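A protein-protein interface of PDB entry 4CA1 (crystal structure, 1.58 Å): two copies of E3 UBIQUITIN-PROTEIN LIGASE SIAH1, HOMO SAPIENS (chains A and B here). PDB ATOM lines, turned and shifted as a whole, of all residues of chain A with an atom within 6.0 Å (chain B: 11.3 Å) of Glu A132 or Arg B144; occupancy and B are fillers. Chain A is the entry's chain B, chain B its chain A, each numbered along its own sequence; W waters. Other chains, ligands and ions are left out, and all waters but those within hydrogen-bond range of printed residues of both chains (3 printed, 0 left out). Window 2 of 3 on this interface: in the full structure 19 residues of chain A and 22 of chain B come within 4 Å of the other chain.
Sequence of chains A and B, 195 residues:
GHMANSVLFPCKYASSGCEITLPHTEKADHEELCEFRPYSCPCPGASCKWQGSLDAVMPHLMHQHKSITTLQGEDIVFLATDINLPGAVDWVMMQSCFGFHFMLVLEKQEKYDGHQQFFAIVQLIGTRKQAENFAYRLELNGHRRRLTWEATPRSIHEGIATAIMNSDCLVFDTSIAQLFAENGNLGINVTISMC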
ATOM      1  N   LEU A 124       7.505  20.366 -11.146  1.00  0.00           N
ATOM      2  CA  LEU A 124       6.366  21.269 -11.307  1.00  0.00           C
ATOM      3  C   LEU A 124       5.542  20.855 -12.530  1.00  0.00           C
ATOM      4  O   LEU A 124       6.108  20.569 -13.604  1.00  0.00           O
ATOM      5  CB  LEU A 124       6.950  22.716 -11.537  1.00  0.00           C
ATOM      6  CG  LEU A 124       5.875  23.759 -11.891  1.00  0.00           C
ATOM      7  CD1 LEU A 124       4.979  24.012 -10.695  1.00  0.00           C
ATOM      8  CD2 LEU A 124       6.521  25.014 -12.434  1.00  0.00           C
ATOM      9  N   THR A 127       6.163  25.005 -16.753  1.00  0.00           N
ATOM     10  CA  THR A 127       7.351  25.135 -17.558  1.00  0.00           C
ATOM     11  C   THR A 127       8.671  25.348 -16.750  1.00  0.00           C
ATOM     12  O   THR A 127       8.654  25.689 -15.565  1.00  0.00           O
ATOM     13  CB  THR A 127       7.159  26.331 -18.503  1.00  0.00           C
ATOM     14  OG1 THR A 127       7.114  27.511 -17.694  1.00  0.00           O
ATOM     15  CG2 THR A 127       5.838  26.179 -19.322  1.00  0.00           C
ATOM     16  N   ARG A 128       9.821  25.166 -17.386  1.00  0.00           N
ATOM     17  CA  ARG A 128      11.123  25.483 -16.711  1.00  0.00           C
ATOM     18  C   ARG A 128      11.161  26.909 -16.213  1.00  0.00           C
ATOM     19  O   ARG A 128      11.723  27.150 -15.145  1.00  0.00           O
ATOM     20  CB  ARG A 128      12.365  25.303 -17.608  1.00  0.00           C
ATOM     21  CG  ARG A 128      12.946  23.910 -17.670  1.00  0.00           C
ATOM     22  CD  ARG A 128      12.539  23.224 -18.968  1.00  0.00           C
ATOM     23  NE  ARG A 128      13.672  22.885 -19.812  1.00  0.00           N
ATOM     24  CZ  ARG A 128      13.912  23.377 -21.034  1.00  0.00           C
ATOM     25  NH1 ARG A 128      13.071  24.250 -21.580  1.00  0.00           N
ATOM     26  NH2 ARG A 128      14.946  22.996 -21.674  1.00  0.00           N
ATOM     27  N   LYS A 129      10.592  27.844 -17.000  1.00  0.00           N
ATOM     28  CA  LYS A 129      10.615  29.220 -16.599  1.00  0.00           C
ATOM     29  C   LYS A 129       9.779  29.372 -15.345  1.00  0.00           C
ATOM     30  O   LYS A 129      10.155  30.113 -14.428  1.00  0.00           O
ATOM     31  CB  LYS A 129      10.078  30.161 -17.700  1.00  0.00           C
ATOM     32  CG  LYS A 129      10.726  31.531 -17.641  1.00  0.00           C
ATOM     33  CD  LYS A 129      10.346  32.359 -18.859  1.00  0.00           C
ATOM     34  CE  LYS A 129       9.083  33.183 -18.615  1.00  0.00           C
ATOM     35  NZ  LYS A 129       9.093  34.462 -19.386  1.00  0.00           N
ATOM     36  N   GLN A 130       8.658  28.661 -15.287  1.00  0.00           N
ATOM     37  CA  GLN A 130       7.830  28.754 -14.088  1.00  0.00           C
ATOM     38  C   GLN A 130       8.526  28.077 -12.899  1.00  0.00           C
ATOM     39  O   GLN A 130       8.463  28.556 -11.790  1.00  0.00           O
ATOM     40  CB  GLN A 130       6.477  28.122 -14.329  1.00  0.00           C
ATOM     41  CG  GLN A 130       5.623  28.890 -15.350  1.00  0.00           C
ATOM     42  CD  GLN A 130       4.344  28.195 -15.736  1.00  0.00           C
ATOM     43  OE1 GLN A 130       4.307  26.975 -15.905  1.00  0.00           O
ATOM     44  NE2 GLN A 130       3.269  28.998 -15.958  1.00  0.00           N
ATOM     45  N   ALA A 131       9.200  26.979 -13.154  1.00  0.00           N
ATOM     46  CA  ALA A 131       9.794  26.214 -12.067  1.00  0.00           C
ATOM     47  C   ALA A 131      10.922  27.044 -11.392  1.00  0.00           C
ATOM     48  O   ALA A 131      11.179  26.891 -10.194  1.00  0.00           O
ATOM     49  CB  ALA A 131      10.363  24.906 -12.613  1.00  0.00           C
ATOM     50  N   GLU A 132      11.596  27.910 -12.165  1.00  0.00           N
ATOM     51  CA  GLU A 132      12.697  28.726 -11.661  1.00  0.00           C
ATOM     52  C   GLU A 132      12.305  29.681 -10.527  1.00  0.00           C
ATOM     53  O   GLU A 132      13.188  30.210  -9.842  1.00  0.00           O
ATOM     54  CB  GLU A 132      13.314  29.556 -12.800  1.00  0.00           C
ATOM     55  CG  GLU A 132      14.237  28.768 -13.701  1.00  0.00           C
ATOM     56  CD  GLU A 132      14.694  29.553 -14.940  1.00  0.00           C
ATOM     57  OE1 GLU A 132      14.726  30.827 -14.910  1.00  0.00           O
ATOM     58  OE2 GLU A 132      15.037  28.886 -15.960  1.00  0.00           O
ATOM     59  N   ASN A 133      11.001  29.973 -10.411  1.00  0.00           N
ATOM     60  CA  ASN A 133      10.541  30.828  -9.345  1.00  0.00           C
ATOM     61  C   ASN A 133      10.292  30.074  -8.035  1.00  0.00           C
ATOM     62  O   ASN A 133       9.915  30.691  -7.035  1.00  0.00           O
ATOM     63  CB  ASN A 133       9.232  31.467  -9.814  1.00  0.00           C
ATOM     64  CG  ASN A 133       9.465  32.347 -11.032  1.00  0.00           C
ATOM     65  OD1 ASN A 133      10.464  33.111 -11.074  1.00  0.00           O
ATOM     66  ND2 ASN A 133       8.655  32.184 -12.052  1.00  0.00           N
ATOM     67  N   PHE A 134      10.545  28.756  -8.024  1.00  0.00           N
ATOM     68  CA  PHE A 134      10.236  27.923  -6.832  1.00  0.00           C
ATOM     69  C   PHE A 134      11.512  27.258  -6.296  1.00  0.00           C
ATOM     70  O   PHE A 134      12.450  26.975  -7.074  1.00  0.00           O
ATOM     71  CB  PHE A 134       9.193  26.853  -7.155  1.00  0.00           C
ATOM     72  CG  PHE A 134       7.835  27.482  -7.460  1.00  0.00           C
ATOM     73  CD1 PHE A 134       7.066  27.992  -6.413  1.00  0.00           C
ATOM     74  CD2 PHE A 134       7.372  27.548  -8.745  1.00  0.00           C
ATOM     75  CE1 PHE A 134       5.800  28.589  -6.686  1.00  0.00           C
ATOM     76  CE2 PHE A 134       6.123  28.144  -9.050  1.00  0.00           C
ATOM     77  CZ  PHE A 134       5.368  28.654  -8.006  1.00  0.00           C
ATOM     78  N   GLU A 150      17.548  20.428  -0.806  1.00  0.00           N
ATOM     79  CA  GLU A 150      16.860  21.593  -1.348  1.00  0.00           C
ATOM     80  C   GLU A 150      17.258  21.813  -2.752  1.00  0.00           C
ATOM     81  O   GLU A 150      18.472  21.754  -3.047  1.00  0.00           O
ATOM     82  CB  GLU A 150      17.239  22.866  -0.483  1.00  0.00           C
ATOM     83  CG  GLU A 150      16.722  22.730   0.928  1.00  0.00           C
ATOM     84  CD  GLU A 150      17.295  23.701   1.899  1.00  0.00           C
ATOM     85  OE1 GLU A 150      18.416  23.492   2.403  1.00  0.00           O
ATOM     86  OE2 GLU A 150      16.617  24.751   2.158  1.00  0.00           O
ATOM     87  N   ALA A 151      16.348  22.151  -3.624  1.00  0.00           N
ATOM     88  CA  ALA A 151      16.697  22.329  -5.035  1.00  0.00           C
ATOM     89  C   ALA A 151      15.539  23.081  -5.729  1.00  0.00           C
ATOM     90  O   ALA A 151      14.517  23.411  -5.126  1.00  0.00           O
ATOM     91  CB  ALA A 151      16.908  20.970  -5.727  1.00  0.00           C
ATOM     92  N   THR A 152      15.744  23.376  -6.973  1.00  0.00           N
ATOM     93  CA  THR A 152      14.663  23.905  -7.852  1.00  0.00           C
ATOM     94  C   THR A 152      13.875  22.709  -8.414  1.00  0.00           C
ATOM     95  O   THR A 152      14.461  21.723  -8.931  1.00  0.00           O
ATOM     96  CB  THR A 152      15.323  24.609  -9.066  1.00  0.00           C
ATOM     97  OG1 THR A 152      16.222  25.643  -8.560  1.00  0.00           O
ATOM     98  CG2 THR A 152      14.231  25.272  -9.930  1.00  0.00           C
ATOM     99  N   PRO A 153      12.541  22.780  -8.387  1.00  0.00           N
ATOM    100  CA  PRO A 153      11.824  21.623  -8.983  1.00  0.00           C
ATOM    101  C   PRO A 153      12.142  21.439 -10.461  1.00  0.00           C
ATOM    102  O   PRO A 153      12.358  22.446 -11.197  1.00  0.00           O
ATOM    103  CB  PRO A 153      10.329  22.029  -8.892  1.00  0.00           C
ATOM    104  CG  PRO A 153      10.248  23.202  -7.995  1.00  0.00           C
ATOM    105  CD  PRO A 153      11.635  23.816  -7.840  1.00  0.00           C
ATOM    106  N   CYS A 195      11.212  31.758  -4.573  1.00  0.00           N
ATOM    107  CA  CYS A 195      12.521  32.424  -4.527  1.00  0.00           C
ATOM    108  C   CYS A 195      12.669  33.537  -5.557  1.00  0.00           C
ATOM    109  O   CYS A 195      11.638  34.118  -5.899  1.00  0.00           O
ATOM    110  CB  CYS A 195      13.694  31.408  -4.584  1.00  0.00           C
ATOM    111  SG  CYS A 195      13.497  30.259  -5.957  1.00  0.00           S
ATOM    112  OXT CYS A 195      13.759  33.873  -6.057  1.00  0.00           O
ATOM    113  N   LEU B 140      26.521  20.417   2.018  1.00  0.00           N
ATOM    114  CA  LEU B 140      27.124  20.592   0.685  1.00  0.00           C
ATOM    115  C   LEU B 140      26.307  21.634  -0.033  1.00  0.00           C
ATOM    116  O   LEU B 140      25.065  21.599   0.021  1.00  0.00           O
ATOM    117  CB  LEU B 140      27.092  19.290  -0.133  1.00  0.00           C
ATOM    118  CG  LEU B 140      27.713  18.034   0.557  1.00  0.00           C
ATOM    119  CD1 LEU B 140      27.673  16.888  -0.489  1.00  0.00           C
ATOM    120  CD2 LEU B 140      29.124  18.270   1.058  1.00  0.00           C
ATOM    121  N   ASN B 141      26.977  22.647  -0.576  1.00  0.00           N
ATOM    122  CA  ASN B 141      26.281  23.739  -1.285  1.00  0.00           C
ATOM    123  C   ASN B 141      26.710  23.839  -2.700  1.00  0.00           C
ATOM    124  O   ASN B 141      27.946  23.790  -2.982  1.00  0.00           O
ATOM    125  CB  ASN B 141      26.667  25.025  -0.574  1.00  0.00           C
ATOM    126  CG  ASN B 141      25.896  25.177   0.685  1.00  0.00           C
ATOM    127  OD1 ASN B 141      24.706  25.473   0.649  1.00  0.00           O
ATOM    128  ND2 ASN B 141      26.536  24.933   1.817  1.00  0.00           N
ATOM    129  N   GLY B 142      25.754  23.998  -3.588  1.00  0.00           N
ATOM    130  CA  GLY B 142      26.051  24.108  -5.028  1.00  0.00           C
ATOM    131  C   GLY B 142      25.084  25.079  -5.621  1.00  0.00           C
ATOM    132  O   GLY B 142      24.352  25.734  -4.865  1.00  0.00           O
ATOM    133  N   HIS B 143      25.104  25.222  -6.938  1.00  0.00           N
ATOM    134  CA  HIS B 143      24.189  26.207  -7.533  1.00  0.00           C
ATOM    135  C   HIS B 143      22.758  25.704  -7.430  1.00  0.00           C
ATOM    136  O   HIS B 143      22.362  24.703  -7.999  1.00  0.00           O
ATOM    137  CB  HIS B 143      24.496  26.670  -8.963  1.00  0.00           C
ATOM    138  CG  HIS B 143      23.562  27.759  -9.436  1.00  0.00           C
ATOM    139  ND1 HIS B 143      22.637  27.575 -10.453  1.00  0.00           N
ATOM    140  CD2 HIS B 143      23.382  29.032  -9.000  1.00  0.00           C
ATOM    141  CE1 HIS B 143      21.951  28.690 -10.636  1.00  0.00           C
ATOM    142  NE2 HIS B 143      22.369  29.584  -9.756  1.00  0.00           N
ATOM    143  N   ARG B 144      21.981  26.444  -6.635  1.00  0.00           N
ATOM    144  CA  ARG B 144      20.560  26.137  -6.421  1.00  0.00           C
ATOM    145  C   ARG B 144      20.365  24.728  -5.854  1.00  0.00           C
ATOM    146  O   ARG B 144      19.348  24.076  -6.113  1.00  0.00           O
ATOM    147  CB  ARG B 144      19.796  26.334  -7.740  1.00  0.00           C
ATOM    148  CG  ARG B 144      19.732  27.811  -8.162  1.00  0.00           C
ATOM    149  CD  ARG B 144      19.102  27.972  -9.525  1.00  0.00           C
ATOM    150  NE  ARG B 144      17.671  28.091  -9.274  1.00  0.00           N
ATOM    151  CZ  ARG B 144      16.866  29.042  -9.773  1.00  0.00           C
ATOM    152  NH1 ARG B 144      17.323  29.928 -10.582  1.00  0.00           N
ATOM    153  NH2 ARG B 144      15.582  29.061  -9.418  1.00  0.00           N
ATOM    154  N   ARG B 145      21.363  24.231  -5.090  1.00  0.00           N
ATOM    155  CA  ARG B 145      21.266  22.892  -4.480  1.00  0.00           C
ATOM    156  C   ARG B 145      21.907  22.903  -3.134  1.00  0.00           C
ATOM    157  O   ARG B 145      22.977  23.546  -2.919  1.00  0.00           O
ATOM    158  CB  ARG B 145      22.000  21.795  -5.291  1.00  0.00           C
ATOM    159  CG  ARG B 145      21.489  21.560  -6.695  1.00  0.00           C
ATOM    160  CD  ARG B 145      22.559  20.748  -7.537  1.00  0.00           C
ATOM    161  NE  ARG B 145      22.001  20.398  -8.833  1.00  0.00           N
ATOM    162  CZ  ARG B 145      22.012  21.173  -9.913  1.00  0.00           C
ATOM    163  NH1 ARG B 145      22.521  22.400  -9.846  1.00  0.00           N
ATOM    164  NH2 ARG B 145      21.480  20.735 -11.069  1.00  0.00           N
ATOM    165  N   ARG B 146      21.324  22.177  -2.191  1.00  0.00           N
ATOM    166  CA  ARG B 146      21.940  22.012  -0.869  1.00  0.00           C
ATOM    167  C   ARG B 146      21.571  20.679  -0.297  1.00  0.00           C
ATOM    168  O   ARG B 146      20.413  20.292  -0.292  1.00  0.00           O
ATOM    169  CB  ARG B 146      21.446  23.134   0.080  1.00  0.00           C
ATOM    170  CG  ARG B 146      22.171  23.057   1.431  1.00  0.00           C
ATOM    171  CD  ARG B 146      21.751  24.121   2.424  1.00  0.00           C
ATOM    172  NE  ARG B 146      22.091  25.391   1.879  1.00  0.00           N
ATOM    173  CZ  ARG B 146      21.177  26.327   1.630  1.00  0.00           C
ATOM    174  NH1 ARG B 146      19.924  26.043   1.843  1.00  0.00           N
ATOM    175  NH2 ARG B 146      21.525  27.499   1.147  1.00  0.00           N
ATOM    176  N   LEU B 147      22.556  19.945   0.201  1.00  0.00           N
ATOM    177  CA  LEU B 147      22.314  18.639   0.871  1.00  0.00           C
ATOM    178  C   LEU B 147      22.834  18.803   2.275  1.00  0.00           C
ATOM    179  O   LEU B 147      24.014  19.206   2.483  1.00  0.00           O
ATOM    180  CB  LEU B 147      23.085  17.529   0.135  1.00  0.00           C
ATOM    181  CG  LEU B 147      23.016  16.122   0.803  1.00  0.00           C
ATOM    182  CD1 LEU B 147      21.570  15.599   0.799  1.00  0.00           C
ATOM    183  CD2 LEU B 147      23.912  15.174  -0.036  1.00  0.00           C
ATOM    184  N   THR B 148      22.001  18.487   3.277  1.00  0.00           N
ATOM    185  CA  THR B 148      22.382  18.702   4.693  1.00  0.00           C
ATOM    186  C   THR B 148      22.149  17.471   5.518  1.00  0.00           C
ATOM    187  O   THR B 148      21.102  16.776   5.368  1.00  0.00           O
ATOM    188  CB  THR B 148      21.476  19.828   5.305  1.00  0.00           C
ATOM    189  OG1 THR B 148      21.531  21.017   4.471  1.00  0.00           O
ATOM    190  CG2 THR B 148      21.964  20.199   6.712  1.00  0.00           C
ATOM    191  N   LEU B 179      28.364  17.165  -8.468  1.00  0.00           N
ATOM    192  CA  LEU B 179      27.405  18.293  -8.456  1.00  0.00           C
ATOM    193  C   LEU B 179      27.864  19.418  -7.575  1.00  0.00           C
ATOM    194  O   LEU B 179      27.589  20.557  -7.870  1.00  0.00           O
ATOM    195  CB  LEU B 179      25.974  17.929  -7.981  1.00  0.00           C
ATOM    196  CG  LEU B 179      25.131  17.093  -8.833  1.00  0.00           C
ATOM    197  CD1 LEU B 179      23.953  16.596  -7.931  1.00  0.00           C
ATOM    198  CD2 LEU B 179      24.727  17.943 -10.032  1.00  0.00           C
ATOM    199  N   PHE B 180      28.559  19.070  -6.483  1.00  0.00           N
ATOM    200  CA  PHE B 180      28.900  20.032  -5.463  1.00  0.00           C
ATOM    201  C   PHE B 180      30.354  20.474  -5.571  1.00  0.00           C
ATOM    202  O   PHE B 180      30.700  21.453  -4.981  1.00  0.00           O
ATOM    203  CB  PHE B 180      28.629  19.475  -4.086  1.00  0.00           C
ATOM    204  CG  PHE B 180      27.114  19.424  -3.820  1.00  0.00           C
ATOM    205  CD1 PHE B 180      26.462  20.599  -3.572  1.00  0.00           C
ATOM    206  CD2 PHE B 180      26.403  18.221  -3.779  1.00  0.00           C
ATOM    207  CE1 PHE B 180      25.089  20.610  -3.294  1.00  0.00           C
ATOM    208  CE2 PHE B 180      24.982  18.224  -3.571  1.00  0.00           C
ATOM    209  CZ  PHE B 180      24.342  19.404  -3.268  1.00  0.00           C
ATOM    210  N   GLU B 182      34.094  21.862  -6.874  1.00  0.00           N
ATOM    211  CA  GLU B 182      34.544  22.896  -7.801  1.00  0.00           C
ATOM    212  C   GLU B 182      36.055  22.744  -7.917  1.00  0.00           C
ATOM    213  O   GLU B 182      36.723  22.595  -6.874  1.00  0.00           O
ATOM    214  CB  GLU B 182      34.350  24.267  -7.195  1.00  0.00           C
ATOM    215  CG  GLU B 182      32.949  24.802  -7.123  1.00  0.00           C
ATOM    216  CD  GLU B 182      32.989  26.270  -7.519  1.00  0.00           C
ATOM    217  OE1 GLU B 182      33.993  26.939  -7.145  1.00  0.00           O
ATOM    218  OE2 GLU B 182      32.058  26.727  -8.225  1.00  0.00           O
HETATM  219  O   HOH W   1      18.352  22.781  -8.395  1.00  0.00           O
HETATM  220  O   HOH W   2      19.567  21.032   2.506  1.00  0.00           O
HETATM  221  O   HOH W   3      15.158  27.430  -7.018  1.00  0.00           O
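Of the 14 printed residues of chain A, 4 touch a printed residue of chain B. Hydrophobic or aromatic side chains of chain A that line the printed part of chain B: Ala A151. Along chain B the printed residues that touch a printed residue of chain A span positions 144 to 146. Among the printed residues, Asp or Glu carboxylates within 4 Å of a Lys or Arg side-chain nitrogen of the other chain: Glu A150 with Arg B146 (3.0 Å).
Glu A150 touches Arg B144 (O to O, 3.9 Å). O of Glu A150 touches CA of Arg B145 (3.3 Å). Ala A151 touches Arg B144 (CA to O, 3.4 Å).
Water W3 lies within hydrogen-bond range of OG1 of Thr A152 (2.6 Å), O of Phe A134 (2.7 Å), NH2 of Arg B144 (2.9 Å) and SG of Cys A195 (3.4 Å). Water W2 lies within hydrogen-bond range of the side-chain carboxylate (OE1) of Glu A150 (2.7 Å), the side-chain hydroxyl (OG1) of Thr B148 (2.8 Å) and the backbone carbonyl oxygen (O) of Arg B146 (3.0 Å). Water W1 lies within hydrogen-bond range of the backbone carbonyl oxygen of Arg B144 (2.8 Å) and the backbone NH of Thr A152 (3.0 Å).
Glu A132 touches one residue of chain B. Ala A131 touches none of the printed residues of chain B. Of chain B, only Arg B144 comes within 4 Å of Ala A151. Thr A152 touches one residue of chain B. No residue of chain B comes within 4 Å of Pro A153. Of the printed residues of chain A, Arg B145 touches Glu A150 (3.3 Å). Of the printed residues of chain A, Arg B146 touches Glu A150. Printed residues of chain B within 4 Å of Glu A150: Arg B144, Arg B145 and Arg B146. Arg A128 touches none of the printed residues of chain B. His B143 touches none of the printed residues of chain A. The nearest residue of chain A that does not touch Arg B144 is Cys A195 (4.2 Å).
The guanidinium group (NE) of Arg B146 lies within hydrogen-bond range of the side-chain amide oxygen (OD1) of Asn B141 (2.9 Å). The guanidinium group of Arg B145 sits at hydrogen-bond distance from the backbone carbonyl oxygen of His B143 (3.0 Å).
The guanidinium group (NH2) of Arg B144 sits at hydrogen-bond distance from the backbone carbonyl oxygen (O) of Glu A132 (2.7 Å). NE of Arg B144 lies within hydrogen-bond range of OG1 of Thr A152. The side-chain carboxylate (OE1) of Glu A150 lies within salt-bridge range of the guanidinium group (NH1) of Arg B146.
No position is printed for both chains. Of the 6 pairs that touch across the chains among the printed residues, none has its exchanged pair printed and touching as well.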
